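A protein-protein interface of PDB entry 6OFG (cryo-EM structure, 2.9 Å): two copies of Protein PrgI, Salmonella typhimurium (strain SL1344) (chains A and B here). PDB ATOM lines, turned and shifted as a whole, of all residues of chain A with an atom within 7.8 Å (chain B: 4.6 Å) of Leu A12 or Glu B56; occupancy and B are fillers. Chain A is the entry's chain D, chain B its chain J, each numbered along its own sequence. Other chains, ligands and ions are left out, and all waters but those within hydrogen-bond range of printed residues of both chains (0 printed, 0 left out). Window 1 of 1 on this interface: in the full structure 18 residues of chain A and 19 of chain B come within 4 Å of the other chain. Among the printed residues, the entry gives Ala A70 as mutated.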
ATOM      1  N   TRP A   8      19.697 -29.527  -8.724  1.00  0.00           N
ATOM      2  CA  TRP A   8      19.354 -28.707  -7.573  1.00  0.00           C
ATOM      3  C   TRP A   8      18.718 -27.400  -8.019  1.00  0.00           C
ATOM      4  O   TRP A   8      19.098 -26.827  -9.042  1.00  0.00           O
ATOM      5  CB  TRP A   8      20.602 -28.412  -6.752  1.00  0.00           C
ATOM      6  CG  TRP A   8      20.310 -27.709  -5.495  1.00  0.00           C
ATOM      7  CD1 TRP A   8      19.781 -28.237  -4.361  1.00  0.00           C
ATOM      8  CD2 TRP A   8      20.456 -26.315  -5.259  1.00  0.00           C
ATOM      9  NE1 TRP A   8      19.628 -27.260  -3.412  1.00  0.00           N
ATOM     10  CE2 TRP A   8      20.031 -26.066  -3.946  1.00  0.00           C
ATOM     11  CE3 TRP A   8      20.918 -25.251  -6.030  1.00  0.00           C
ATOM     12  CZ2 TRP A   8      20.053 -24.798  -3.389  1.00  0.00           C
ATOM     13  CZ3 TRP A   8      20.938 -24.003  -5.477  1.00  0.00           C
ATOM     14  CH2 TRP A   8      20.513 -23.782  -4.169  1.00  0.00           C
ATOM     15  N   SER A   9      17.744 -26.925  -7.247  1.00  0.00           N
ATOM     16  CA  SER A   9      17.095 -25.648  -7.514  1.00  0.00           C
ATOM     17  C   SER A   9      16.823 -24.948  -6.196  1.00  0.00           C
ATOM     18  O   SER A   9      16.160 -25.508  -5.320  1.00  0.00           O
ATOM     19  CB  SER A   9      15.796 -25.836  -8.295  1.00  0.00           C
ATOM     20  OG  SER A   9      16.061 -26.323  -9.596  1.00  0.00           O
ATOM     21  N   GLY A  10      17.333 -23.730  -6.058  1.00  0.00           N
ATOM     22  CA  GLY A  10      17.084 -22.927  -4.885  1.00  0.00           C
ATOM     23  C   GLY A  10      15.782 -22.170  -5.000  1.00  0.00           C
ATOM     24  O   GLY A  10      14.946 -22.429  -5.862  1.00  0.00           O
ATOM     25  N   TYR A  11      15.615 -21.199  -4.104  1.00  0.00           N
ATOM     26  CA  TYR A  11      14.371 -20.441  -4.079  1.00  0.00           C
ATOM     27  C   TYR A  11      14.293 -19.455  -5.231  1.00  0.00           C
ATOM     28  O   TYR A  11      13.199 -19.178  -5.728  1.00  0.00           O
ATOM     29  CB  TYR A  11      14.227 -19.708  -2.754  1.00  0.00           C
ATOM     30  CG  TYR A  11      12.916 -18.987  -2.589  1.00  0.00           C
ATOM     31  CD1 TYR A  11      11.764 -19.680  -2.258  1.00  0.00           C
ATOM     32  CD2 TYR A  11      12.828 -17.618  -2.767  1.00  0.00           C
ATOM     33  CE1 TYR A  11      10.563 -19.027  -2.107  1.00  0.00           C
ATOM     34  CE2 TYR A  11      11.633 -16.960  -2.625  1.00  0.00           C
ATOM     35  CZ  TYR A  11      10.507 -17.667  -2.292  1.00  0.00           C
ATOM     36  OH  TYR A  11       9.315 -17.008  -2.144  1.00  0.00           O
ATOM     37  N   LEU A  12      15.427 -18.906  -5.665  1.00  0.00           N
ATOM     38  CA  LEU A  12      15.407 -18.040  -6.836  1.00  0.00           C
ATOM     39  C   LEU A  12      15.210 -18.845  -8.104  1.00  0.00           C
ATOM     40  O   LEU A  12      14.639 -18.341  -9.073  1.00  0.00           O
ATOM     41  CB  LEU A  12      16.695 -17.236  -6.931  1.00  0.00           C
ATOM     42  CG  LEU A  12      16.942 -16.321  -5.746  1.00  0.00           C
ATOM     43  CD1 LEU A  12      18.249 -15.623  -5.914  1.00  0.00           C
ATOM     44  CD2 LEU A  12      15.832 -15.335  -5.637  1.00  0.00           C
ATOM     45  N   ASP A  13      15.679 -20.090  -8.114  1.00  0.00           N
ATOM     46  CA  ASP A  13      15.426 -20.970  -9.243  1.00  0.00           C
ATOM     47  C   ASP A  13      13.962 -21.349  -9.322  1.00  0.00           C
ATOM     48  O   ASP A  13      13.422 -21.489 -10.419  1.00  0.00           O
ATOM     49  CB  ASP A  13      16.281 -22.220  -9.131  1.00  0.00           C
ATOM     50  CG  ASP A  13      17.745 -21.925  -9.235  1.00  0.00           C
ATOM     51  OD1 ASP A  13      18.108 -20.960  -9.930  1.00  0.00           O
ATOM     52  OD2 ASP A  13      18.535 -22.651  -8.606  1.00  0.00           O
ATOM     53  N   ASP A  14      13.305 -21.508  -8.176  1.00  0.00           N
ATOM     54  CA  ASP A  14      11.893 -21.856  -8.182  1.00  0.00           C
ATOM     55  C   ASP A  14      11.029 -20.670  -8.588  1.00  0.00           C
ATOM     56  O   ASP A  14      10.018 -20.845  -9.270  1.00  0.00           O
ATOM     57  CB  ASP A  14      11.485 -22.381  -6.811  1.00  0.00           C
ATOM     58  CG  ASP A  14      12.150 -23.695  -6.477  1.00  0.00           C
ATOM     59  OD1 ASP A  14      12.496 -24.436  -7.418  1.00  0.00           O
ATOM     60  OD2 ASP A  14      12.327 -23.989  -5.278  1.00  0.00           O
ATOM     61  N   VAL A  15      11.411 -19.459  -8.179  1.00  0.00           N
ATOM     62  CA  VAL A  15      10.686 -18.261  -8.596  1.00  0.00           C
ATOM     63  C   VAL A  15      10.885 -18.006 -10.085  1.00  0.00           C
ATOM     64  O   VAL A  15       9.932 -17.696 -10.808  1.00  0.00           O
ATOM     65  CB  VAL A  15      11.122 -17.058  -7.738  1.00  0.00           C
ATOM     66  CG1 VAL A  15      10.581 -15.766  -8.292  1.00  0.00           C
ATOM     67  CG2 VAL A  15      10.631 -17.227  -6.320  1.00  0.00           C
ATOM     68  N   SER A  16      12.111 -18.180 -10.577  1.00  0.00           N
ATOM     69  CA  SER A  16      12.381 -18.012 -11.999  1.00  0.00           C
ATOM     70  C   SER A  16      11.783 -19.127 -12.846  1.00  0.00           C
ATOM     71  O   SER A  16      11.635 -18.949 -14.056  1.00  0.00           O
ATOM     72  CB  SER A  16      13.885 -17.931 -12.238  1.00  0.00           C
ATOM     73  OG  SER A  16      14.184 -17.761 -13.607  1.00  0.00           O
ATOM     74  N   ALA A  17      11.444 -20.269 -12.252  1.00  0.00           N
ATOM     75  CA  ALA A  17      10.771 -21.332 -12.981  1.00  0.00           C
ATOM     76  C   ALA A  17       9.262 -21.320 -12.802  1.00  0.00           C
ATOM     77  O   ALA A  17       8.575 -22.072 -13.495  1.00  0.00           O
ATOM     78  CB  ALA A  17      11.310 -22.701 -12.568  1.00  0.00           C
ATOM     79  N   LYS A  18       8.726 -20.515 -11.885  1.00  0.00           N
ATOM     80  CA  LYS A  18       7.291 -20.268 -11.913  1.00  0.00           C
ATOM     81  C   LYS A  18       6.912 -19.473 -13.150  1.00  0.00           C
ATOM     82  O   LYS A  18       5.886 -19.745 -13.775  1.00  0.00           O
ATOM     83  CB  LYS A  18       6.836 -19.541 -10.648  1.00  0.00           C
ATOM     84  CG  LYS A  18       6.788 -20.400  -9.402  1.00  0.00           C
ATOM     85  CD  LYS A  18       6.321 -19.590  -8.206  1.00  0.00           C
ATOM     86  CE  LYS A  18       6.352 -20.410  -6.923  1.00  0.00           C
ATOM     87  NZ  LYS A  18       5.930 -19.621  -5.726  1.00  0.00           N
ATOM     88  N   PHE A  19       7.742 -18.496 -13.524  1.00  0.00           N
ATOM     89  CA  PHE A  19       7.568 -17.802 -14.793  1.00  0.00           C
ATOM     90  C   PHE A  19       7.783 -18.728 -15.980  1.00  0.00           C
ATOM     91  O   PHE A  19       7.087 -18.594 -16.987  1.00  0.00           O
ATOM     92  CB  PHE A  19       8.527 -16.614 -14.889  1.00  0.00           C
ATOM     93  CG  PHE A  19       8.162 -15.459 -14.007  1.00  0.00           C
ATOM     94  CD1 PHE A  19       7.190 -14.555 -14.399  1.00  0.00           C
ATOM     95  CD2 PHE A  19       8.803 -15.263 -12.799  1.00  0.00           C
ATOM     96  CE1 PHE A  19       6.859 -13.489 -13.596  1.00  0.00           C
ATOM     97  CE2 PHE A  19       8.472 -14.199 -11.994  1.00  0.00           C
ATOM     98  CZ  PHE A  19       7.500 -13.314 -12.393  1.00  0.00           C
ATOM     99  N   GLN A  64      10.375 -11.664 -14.950  1.00  0.00           N
ATOM    100  CA  GLN A  64      11.148 -12.760 -14.387  1.00  0.00           C
ATOM    101  C   GLN A  64      12.445 -12.254 -13.784  1.00  0.00           C
ATOM    102  O   GLN A  64      12.850 -12.696 -12.707  1.00  0.00           O
ATOM    103  CB  GLN A  64      11.453 -13.795 -15.458  1.00  0.00           C
ATOM    104  CG  GLN A  64      12.087 -15.053 -14.934  1.00  0.00           C
ATOM    105  CD  GLN A  64      12.483 -15.981 -16.039  1.00  0.00           C
ATOM    106  OE1 GLN A  64      12.429 -15.620 -17.205  1.00  0.00           O
ATOM    107  NE2 GLN A  64      12.865 -17.192 -15.687  1.00  0.00           N
ATOM    108  N   THR A  67      12.011 -10.002 -10.562  1.00  0.00           N
ATOM    109  CA  THR A  67      11.514 -10.698  -9.389  1.00  0.00           C
ATOM    110  C   THR A  67      12.613 -11.519  -8.732  1.00  0.00           C
ATOM    111  O   THR A  67      12.681 -11.595  -7.502  1.00  0.00           O
ATOM    112  CB  THR A  67      10.335 -11.583  -9.779  1.00  0.00           C
ATOM    113  OG1 THR A  67       9.369 -10.784 -10.465  1.00  0.00           O
ATOM    114  CG2 THR A  67       9.671 -12.163  -8.568  1.00  0.00           C
ATOM    115  N   VAL A  68      13.491 -12.119  -9.534  1.00  0.00           N
ATOM    116  CA  VAL A  68      14.670 -12.784  -8.991  1.00  0.00           C
ATOM    117  C   VAL A  68      15.598 -11.767  -8.343  1.00  0.00           C
ATOM    118  O   VAL A  68      16.189 -12.028  -7.291  1.00  0.00           O
ATOM    119  CB  VAL A  68      15.366 -13.592 -10.102  1.00  0.00           C
ATOM    120  CG1 VAL A  68      16.645 -14.231  -9.616  1.00  0.00           C
ATOM    121  CG2 VAL A  68      14.442 -14.653 -10.598  1.00  0.00           C
ATOM    122  N   LYS A  69      15.696 -10.572  -8.924  1.00  0.00           N
ATOM    123  CA  LYS A  69      16.502  -9.521  -8.320  1.00  0.00           C
ATOM    124  C   LYS A  69      15.848  -8.974  -7.059  1.00  0.00           C
ATOM    125  O   LYS A  69      16.547  -8.562  -6.129  1.00  0.00           O
ATOM    126  CB  LYS A  69      16.739  -8.402  -9.333  1.00  0.00           C
ATOM    127  CG  LYS A  69      17.711  -7.349  -8.868  1.00  0.00           C
ATOM    128  CD  LYS A  69      19.091  -7.946  -8.776  1.00  0.00           C
ATOM    129  CE  LYS A  69      20.097  -6.945  -8.274  1.00  0.00           C
ATOM    130  NZ  LYS A  69      19.872  -6.645  -6.842  1.00  0.00           N
ATOM    131  N   ALA A  70      14.518  -8.989  -6.994  1.00  0.00           N
ATOM    132  CA  ALA A  70      13.830  -8.457  -5.825  1.00  0.00           C
ATOM    133  C   ALA A  70      13.979  -9.377  -4.625  1.00  0.00           C
ATOM    134  O   ALA A  70      14.222  -8.915  -3.508  1.00  0.00           O
ATOM    135  CB  ALA A  70      12.359  -8.231  -6.140  1.00  0.00           C
ATOM    136  N   PHE A  71      13.833 -10.686  -4.831  1.00  0.00           N
ATOM    137  CA  PHE A  71      14.040 -11.626  -3.738  1.00  0.00           C
ATOM    138  C   PHE A  71      15.502 -11.766  -3.357  1.00  0.00           C
ATOM    139  O   PHE A  71      15.790 -12.082  -2.202  1.00  0.00           O
ATOM    140  CB  PHE A  71      13.476 -12.998  -4.085  1.00  0.00           C
ATOM    141  CG  PHE A  71      11.996 -13.094  -3.960  1.00  0.00           C
ATOM    142  CD1 PHE A  71      11.416 -13.299  -2.727  1.00  0.00           C
ATOM    143  CD2 PHE A  71      11.185 -12.992  -5.069  1.00  0.00           C
ATOM    144  CE1 PHE A  71      10.056 -13.394  -2.600  1.00  0.00           C
ATOM    145  CE2 PHE A  71       9.825 -13.085  -4.948  1.00  0.00           C
ATOM    146  CZ  PHE A  71       9.261 -13.289  -3.713  1.00  0.00           C
ATOM    147  N   LYS A  72      16.428 -11.545  -4.287  1.00  0.00           N
ATOM    148  CA  LYS A  72      17.839 -11.565  -3.929  1.00  0.00           C
ATOM    149  C   LYS A  72      18.199 -10.367  -3.059  1.00  0.00           C
ATOM    150  O   LYS A  72      19.108 -10.455  -2.229  1.00  0.00           O
ATOM    151  CB  LYS A  72      18.691 -11.602  -5.199  1.00  0.00           C
ATOM    152  CG  LYS A  72      20.166 -11.891  -5.007  1.00  0.00           C
ATOM    153  CD  LYS A  72      21.001 -10.636  -5.076  1.00  0.00           C
ATOM    154  CE  LYS A  72      22.469 -10.958  -5.009  1.00  0.00           C
ATOM    155  NZ  LYS A  72      22.899 -11.677  -6.233  1.00  0.00           N
ATOM    156  N   ASP A  73      17.493  -9.251  -3.225  1.00  0.00           N
ATOM    157  CA  ASP A  73      17.710  -8.103  -2.356  1.00  0.00           C
ATOM    158  C   ASP A  73      17.091  -8.312  -0.983  1.00  0.00           C
ATOM    159  O   ASP A  73      17.577  -7.750   0.002  1.00  0.00           O
ATOM    160  CB  ASP A  73      17.141  -6.847  -3.004  1.00  0.00           C
ATOM    161  CG  ASP A  73      17.925  -6.422  -4.222  1.00  0.00           C
ATOM    162  OD1 ASP A  73      19.132  -6.731  -4.281  1.00  0.00           O
ATOM    163  OD2 ASP A  73      17.339  -5.770  -5.115  1.00  0.00           O
ATOM    164  N   ASP A  75      16.959 -11.349   0.451  1.00  0.00           N
ATOM    165  CA  ASP A  75      17.769 -12.373   1.096  1.00  0.00           C
ATOM    166  C   ASP A  75      19.111 -11.827   1.547  1.00  0.00           C
ATOM    167  O   ASP A  75      19.602 -12.192   2.618  1.00  0.00           O
ATOM    168  CB  ASP A  75      17.989 -13.527   0.136  1.00  0.00           C
ATOM    169  CG  ASP A  75      16.728 -14.258  -0.186  1.00  0.00           C
ATOM    170  OD1 ASP A  75      15.851 -14.347   0.689  1.00  0.00           O
ATOM    171  OD2 ASP A  75      16.604 -14.724  -1.331  1.00  0.00           O
ATOM    172  N   LEU B  26      25.632 -26.779  -7.201  1.00  0.00           N
ATOM    173  CA  LEU B  26      25.520 -25.362  -7.521  1.00  0.00           C
ATOM    174  C   LEU B  26      26.863 -24.771  -7.920  1.00  0.00           C
ATOM    175  O   LEU B  26      26.913 -23.855  -8.745  1.00  0.00           O
ATOM    176  CB  LEU B  26      24.932 -24.603  -6.335  1.00  0.00           C
ATOM    177  CG  LEU B  26      24.690 -23.099  -6.471  1.00  0.00           C
ATOM    178  CD1 LEU B  26      23.712 -22.803  -7.579  1.00  0.00           C
ATOM    179  CD2 LEU B  26      24.194 -22.532  -5.174  1.00  0.00           C
ATOM    180  N   SER B  52      19.579 -16.424 -12.404  1.00  0.00           N
ATOM    181  CA  SER B  52      19.041 -17.202 -11.304  1.00  0.00           C
ATOM    182  C   SER B  52      20.071 -18.132 -10.678  1.00  0.00           C
ATOM    183  O   SER B  52      19.887 -18.537  -9.532  1.00  0.00           O
ATOM    184  CB  SER B  52      17.841 -18.005 -11.782  1.00  0.00           C
ATOM    185  OG  SER B  52      17.328 -18.791 -10.732  1.00  0.00           O
ATOM    186  N   LYS B  53      21.142 -18.482 -11.390  1.00  0.00           N
ATOM    187  CA  LYS B  53      22.206 -19.288 -10.800  1.00  0.00           C
ATOM    188  C   LYS B  53      23.226 -18.449 -10.051  1.00  0.00           C
ATOM    189  O   LYS B  53      23.658 -18.835  -8.963  1.00  0.00           O
ATOM    190  CB  LYS B  53      22.931 -20.105 -11.873  1.00  0.00           C
ATOM    191  CG  LYS B  53      22.147 -21.225 -12.537  1.00  0.00           C
ATOM    192  CD  LYS B  53      22.045 -22.467 -11.673  1.00  0.00           C
ATOM    193  CE  LYS B  53      20.691 -22.613 -11.030  1.00  0.00           C
ATOM    194  NZ  LYS B  53      20.562 -23.871 -10.251  1.00  0.00           N
ATOM    195  N   LEU B  54      23.637 -17.320 -10.624  1.00  0.00           N
ATOM    196  CA  LEU B  54      24.645 -16.484  -9.985  1.00  0.00           C
ATOM    197  C   LEU B  54      24.086 -15.785  -8.756  1.00  0.00           C
ATOM    198  O   LEU B  54      24.808 -15.570  -7.777  1.00  0.00           O
ATOM    199  CB  LEU B  54      25.179 -15.472 -10.990  1.00  0.00           C
ATOM    200  CG  LEU B  54      26.280 -14.509 -10.582  1.00  0.00           C
ATOM    201  CD1 LEU B  54      27.498 -15.276 -10.150  1.00  0.00           C
ATOM    202  CD2 LEU B  54      26.599 -13.624 -11.760  1.00  0.00           C
ATOM    203  N   SER B  55      22.804 -15.428  -8.782  1.00  0.00           N
ATOM    204  CA  SER B  55      22.181 -14.849  -7.602  1.00  0.00           C
ATOM    205  C   SER B  55      21.954 -15.898  -6.528  1.00  0.00           C
ATOM    206  O   SER B  55      21.955 -15.577  -5.339  1.00  0.00           O
ATOM    207  CB  SER B  55      20.861 -14.188  -7.974  1.00  0.00           C
ATOM    208  OG  SER B  55      21.062 -13.146  -8.907  1.00  0.00           O
ATOM    209  N   GLU B  56      21.759 -17.150  -6.929  1.00  0.00           N
ATOM    210  CA  GLU B  56      21.615 -18.229  -5.963  1.00  0.00           C
ATOM    211  C   GLU B  56      22.962 -18.591  -5.356  1.00  0.00           C
ATOM    212  O   GLU B  56      23.039 -19.039  -4.209  1.00  0.00           O
ATOM    213  CB  GLU B  56      20.991 -19.435  -6.653  1.00  0.00           C
ATOM    214  CG  GLU B  56      20.607 -20.549  -5.752  1.00  0.00           C
ATOM    215  CD  GLU B  56      19.388 -20.238  -4.937  1.00  0.00           C
ATOM    216  OE1 GLU B  56      18.514 -19.519  -5.443  1.00  0.00           O
ATOM    217  OE2 GLU B  56      19.309 -20.692  -3.777  1.00  0.00           O
ATOM    218  N   TYR B  57      24.035 -18.398  -6.115  1.00  0.00           N
ATOM    219  CA  TYR B  57      25.381 -18.683  -5.645  1.00  0.00           C
ATOM    220  C   TYR B  57      25.911 -17.568  -4.761  1.00  0.00           C
ATOM    221  O   TYR B  57      26.736 -17.817  -3.880  1.00  0.00           O
ATOM    222  CB  TYR B  57      26.294 -18.880  -6.849  1.00  0.00           C
ATOM    223  CG  TYR B  57      27.689 -19.340  -6.548  1.00  0.00           C
ATOM    224  CD1 TYR B  57      27.948 -20.668  -6.262  1.00  0.00           C
ATOM    225  CD2 TYR B  57      28.753 -18.455  -6.571  1.00  0.00           C
ATOM    226  CE1 TYR B  57      29.220 -21.099  -6.000  1.00  0.00           C
ATOM    227  CE2 TYR B  57      30.029 -18.876  -6.306  1.00  0.00           C
ATOM    228  CZ  TYR B  57      30.255 -20.201  -6.021  1.00  0.00           C
ATOM    229  OH  TYR B  57      31.527 -20.638  -5.755  1.00  0.00           O
ATOM    230  N   ASN B  58      25.465 -16.336  -4.999  1.00  0.00           N
ATOM    231  CA  ASN B  58      25.851 -15.220  -4.148  1.00  0.00           C
ATOM    232  C   ASN B  58      25.218 -15.351  -2.769  1.00  0.00           C
ATOM    233  O   ASN B  58      25.846 -15.028  -1.757  1.00  0.00           O
ATOM    234  CB  ASN B  58      25.445 -13.909  -4.822  1.00  0.00           C
ATOM    235  CG  ASN B  58      26.094 -12.693  -4.203  1.00  0.00           C
ATOM    236  OD1 ASN B  58      26.820 -12.782  -3.221  1.00  0.00           O
ATOM    237  ND2 ASN B  58      25.854 -11.540  -4.803  1.00  0.00           N
ATOM    238  N   LEU B  59      23.983 -15.837  -2.707  1.00  0.00           N
ATOM    239  CA  LEU B  59      23.330 -16.016  -1.422  1.00  0.00           C
ATOM    240  C   LEU B  59      23.836 -17.252  -0.707  1.00  0.00           C
ATOM    241  O   LEU B  59      23.826 -17.299   0.525  1.00  0.00           O
ATOM    242  CB  LEU B  59      21.825 -16.106  -1.619  1.00  0.00           C
ATOM    243  CG  LEU B  59      21.222 -14.837  -2.195  1.00  0.00           C
ATOM    244  CD1 LEU B  59      19.789 -15.107  -2.525  1.00  0.00           C
ATOM    245  CD2 LEU B  59      21.359 -13.682  -1.234  1.00  0.00           C
ATOM    246  N   TYR B  60      24.261 -18.256  -1.466  1.00  0.00           N
ATOM    247  CA  TYR B  60      24.895 -19.432  -0.887  1.00  0.00           C
ATOM    248  C   TYR B  60      26.225 -19.091  -0.234  1.00  0.00           C
ATOM    249  O   TYR B  60      26.504 -19.540   0.879  1.00  0.00           O
ATOM    250  CB  TYR B  60      25.053 -20.498  -1.969  1.00  0.00           C
ATOM    251  CG  TYR B  60      26.165 -21.475  -1.737  1.00  0.00           C
ATOM    252  CD1 TYR B  60      26.124 -22.402  -0.705  1.00  0.00           C
ATOM    253  CD2 TYR B  60      27.250 -21.493  -2.593  1.00  0.00           C
ATOM    254  CE1 TYR B  60      27.159 -23.283  -0.513  1.00  0.00           C
ATOM    255  CE2 TYR B  60      28.271 -22.372  -2.420  1.00  0.00           C
ATOM    256  CZ  TYR B  60      28.225 -23.263  -1.383  1.00  0.00           C
ATOM    257  OH  TYR B  60      29.267 -24.132  -1.234  1.00  0.00           O
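OG of Ser B52 sits at hydrogen-bond distance from O of Leu A12 (3.2 Å).
OD1 of Asp A13 sits at hydrogen-bond distance from OG of Ser B52, at 2.4 Å.
NZ of Lys B53 lies within salt-bridge range of OD2 of Asp A13.
The side-chain carboxylate (OE1) of Glu B56 is in hydrogen-bond range of the backbone NH (N) of Leu A12 (3.2 Å).
ND2 of Asn B58 lies close to NZ of Lys A72 (3.3 Å).
The backbone NH of Gly A10 sits at hydrogen-bond distance from the side-chain carboxylate of Asp A13 (3.0 Å).
NE2 of Gln A64 lies within hydrogen-bond range of OG of Ser A16, 2.5 Å away.
Among the printed residues, pairs that only touch across the chains: Trp A8 with Glu B56 (3.3 Å), Gly A10 with Glu B56 (3.3 Å), Asp A75 with Leu B59 (3.4 Å), Trp A8 with Lys B53 (3.5 Å), Lys A72 with Ser B55 (3.5 Å), Trp A8 with Leu B26 (3.6 Å), Tyr A11 with Glu B56 (3.6 Å), Leu A12 with Ser B55 (3.6 Å), Leu A12 with Leu B59 (3.8 Å), Ser A16 with Ser B52 (3.9 Å) and Asp A13 with Glu B56 (3.9 Å).
Leu A12 touches just these residues of chain B: Ser B52 (3.2 Å), Ser B55 (3.6 Å), Glu B56 (3.2 Å) and Leu B59 (3.8 Å).
Of chain A, only Trp A8, Gly A10, Tyr A11, Leu A12 and Asp A13 come within 4 Å of Glu B56.
Printed residues of chain B within 4 Å of Trp A8: Leu B26, Lys B53 and Glu B56.
Printed residues of chain B within 4 Å of Asp A75: Leu B59.
Printed residues of chain B within 4 Å of Asp A13: Ser B52, Lys B53 and Glu B56.
The nearest printed residue of chain B that does not touch Asp A13 is Leu B26 (5.3 Å).
Of the 21 printed residues of chain A, 8 touch a printed residue of chain B.
Hydrophobic or aromatic side chains of chain B that line the printed part of chain A: Leu B26 and Leu B59.
Among the printed residues, Asp or Glu carboxylates within 4 Å of a Lys or Arg side-chain nitrogen of the other chain: Asp A13 with Lys B53.
No position is printed for both chains.
Of the 16 pairs that touch across the chains among the printed residues, none has its exchanged pair printed and touching as well.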
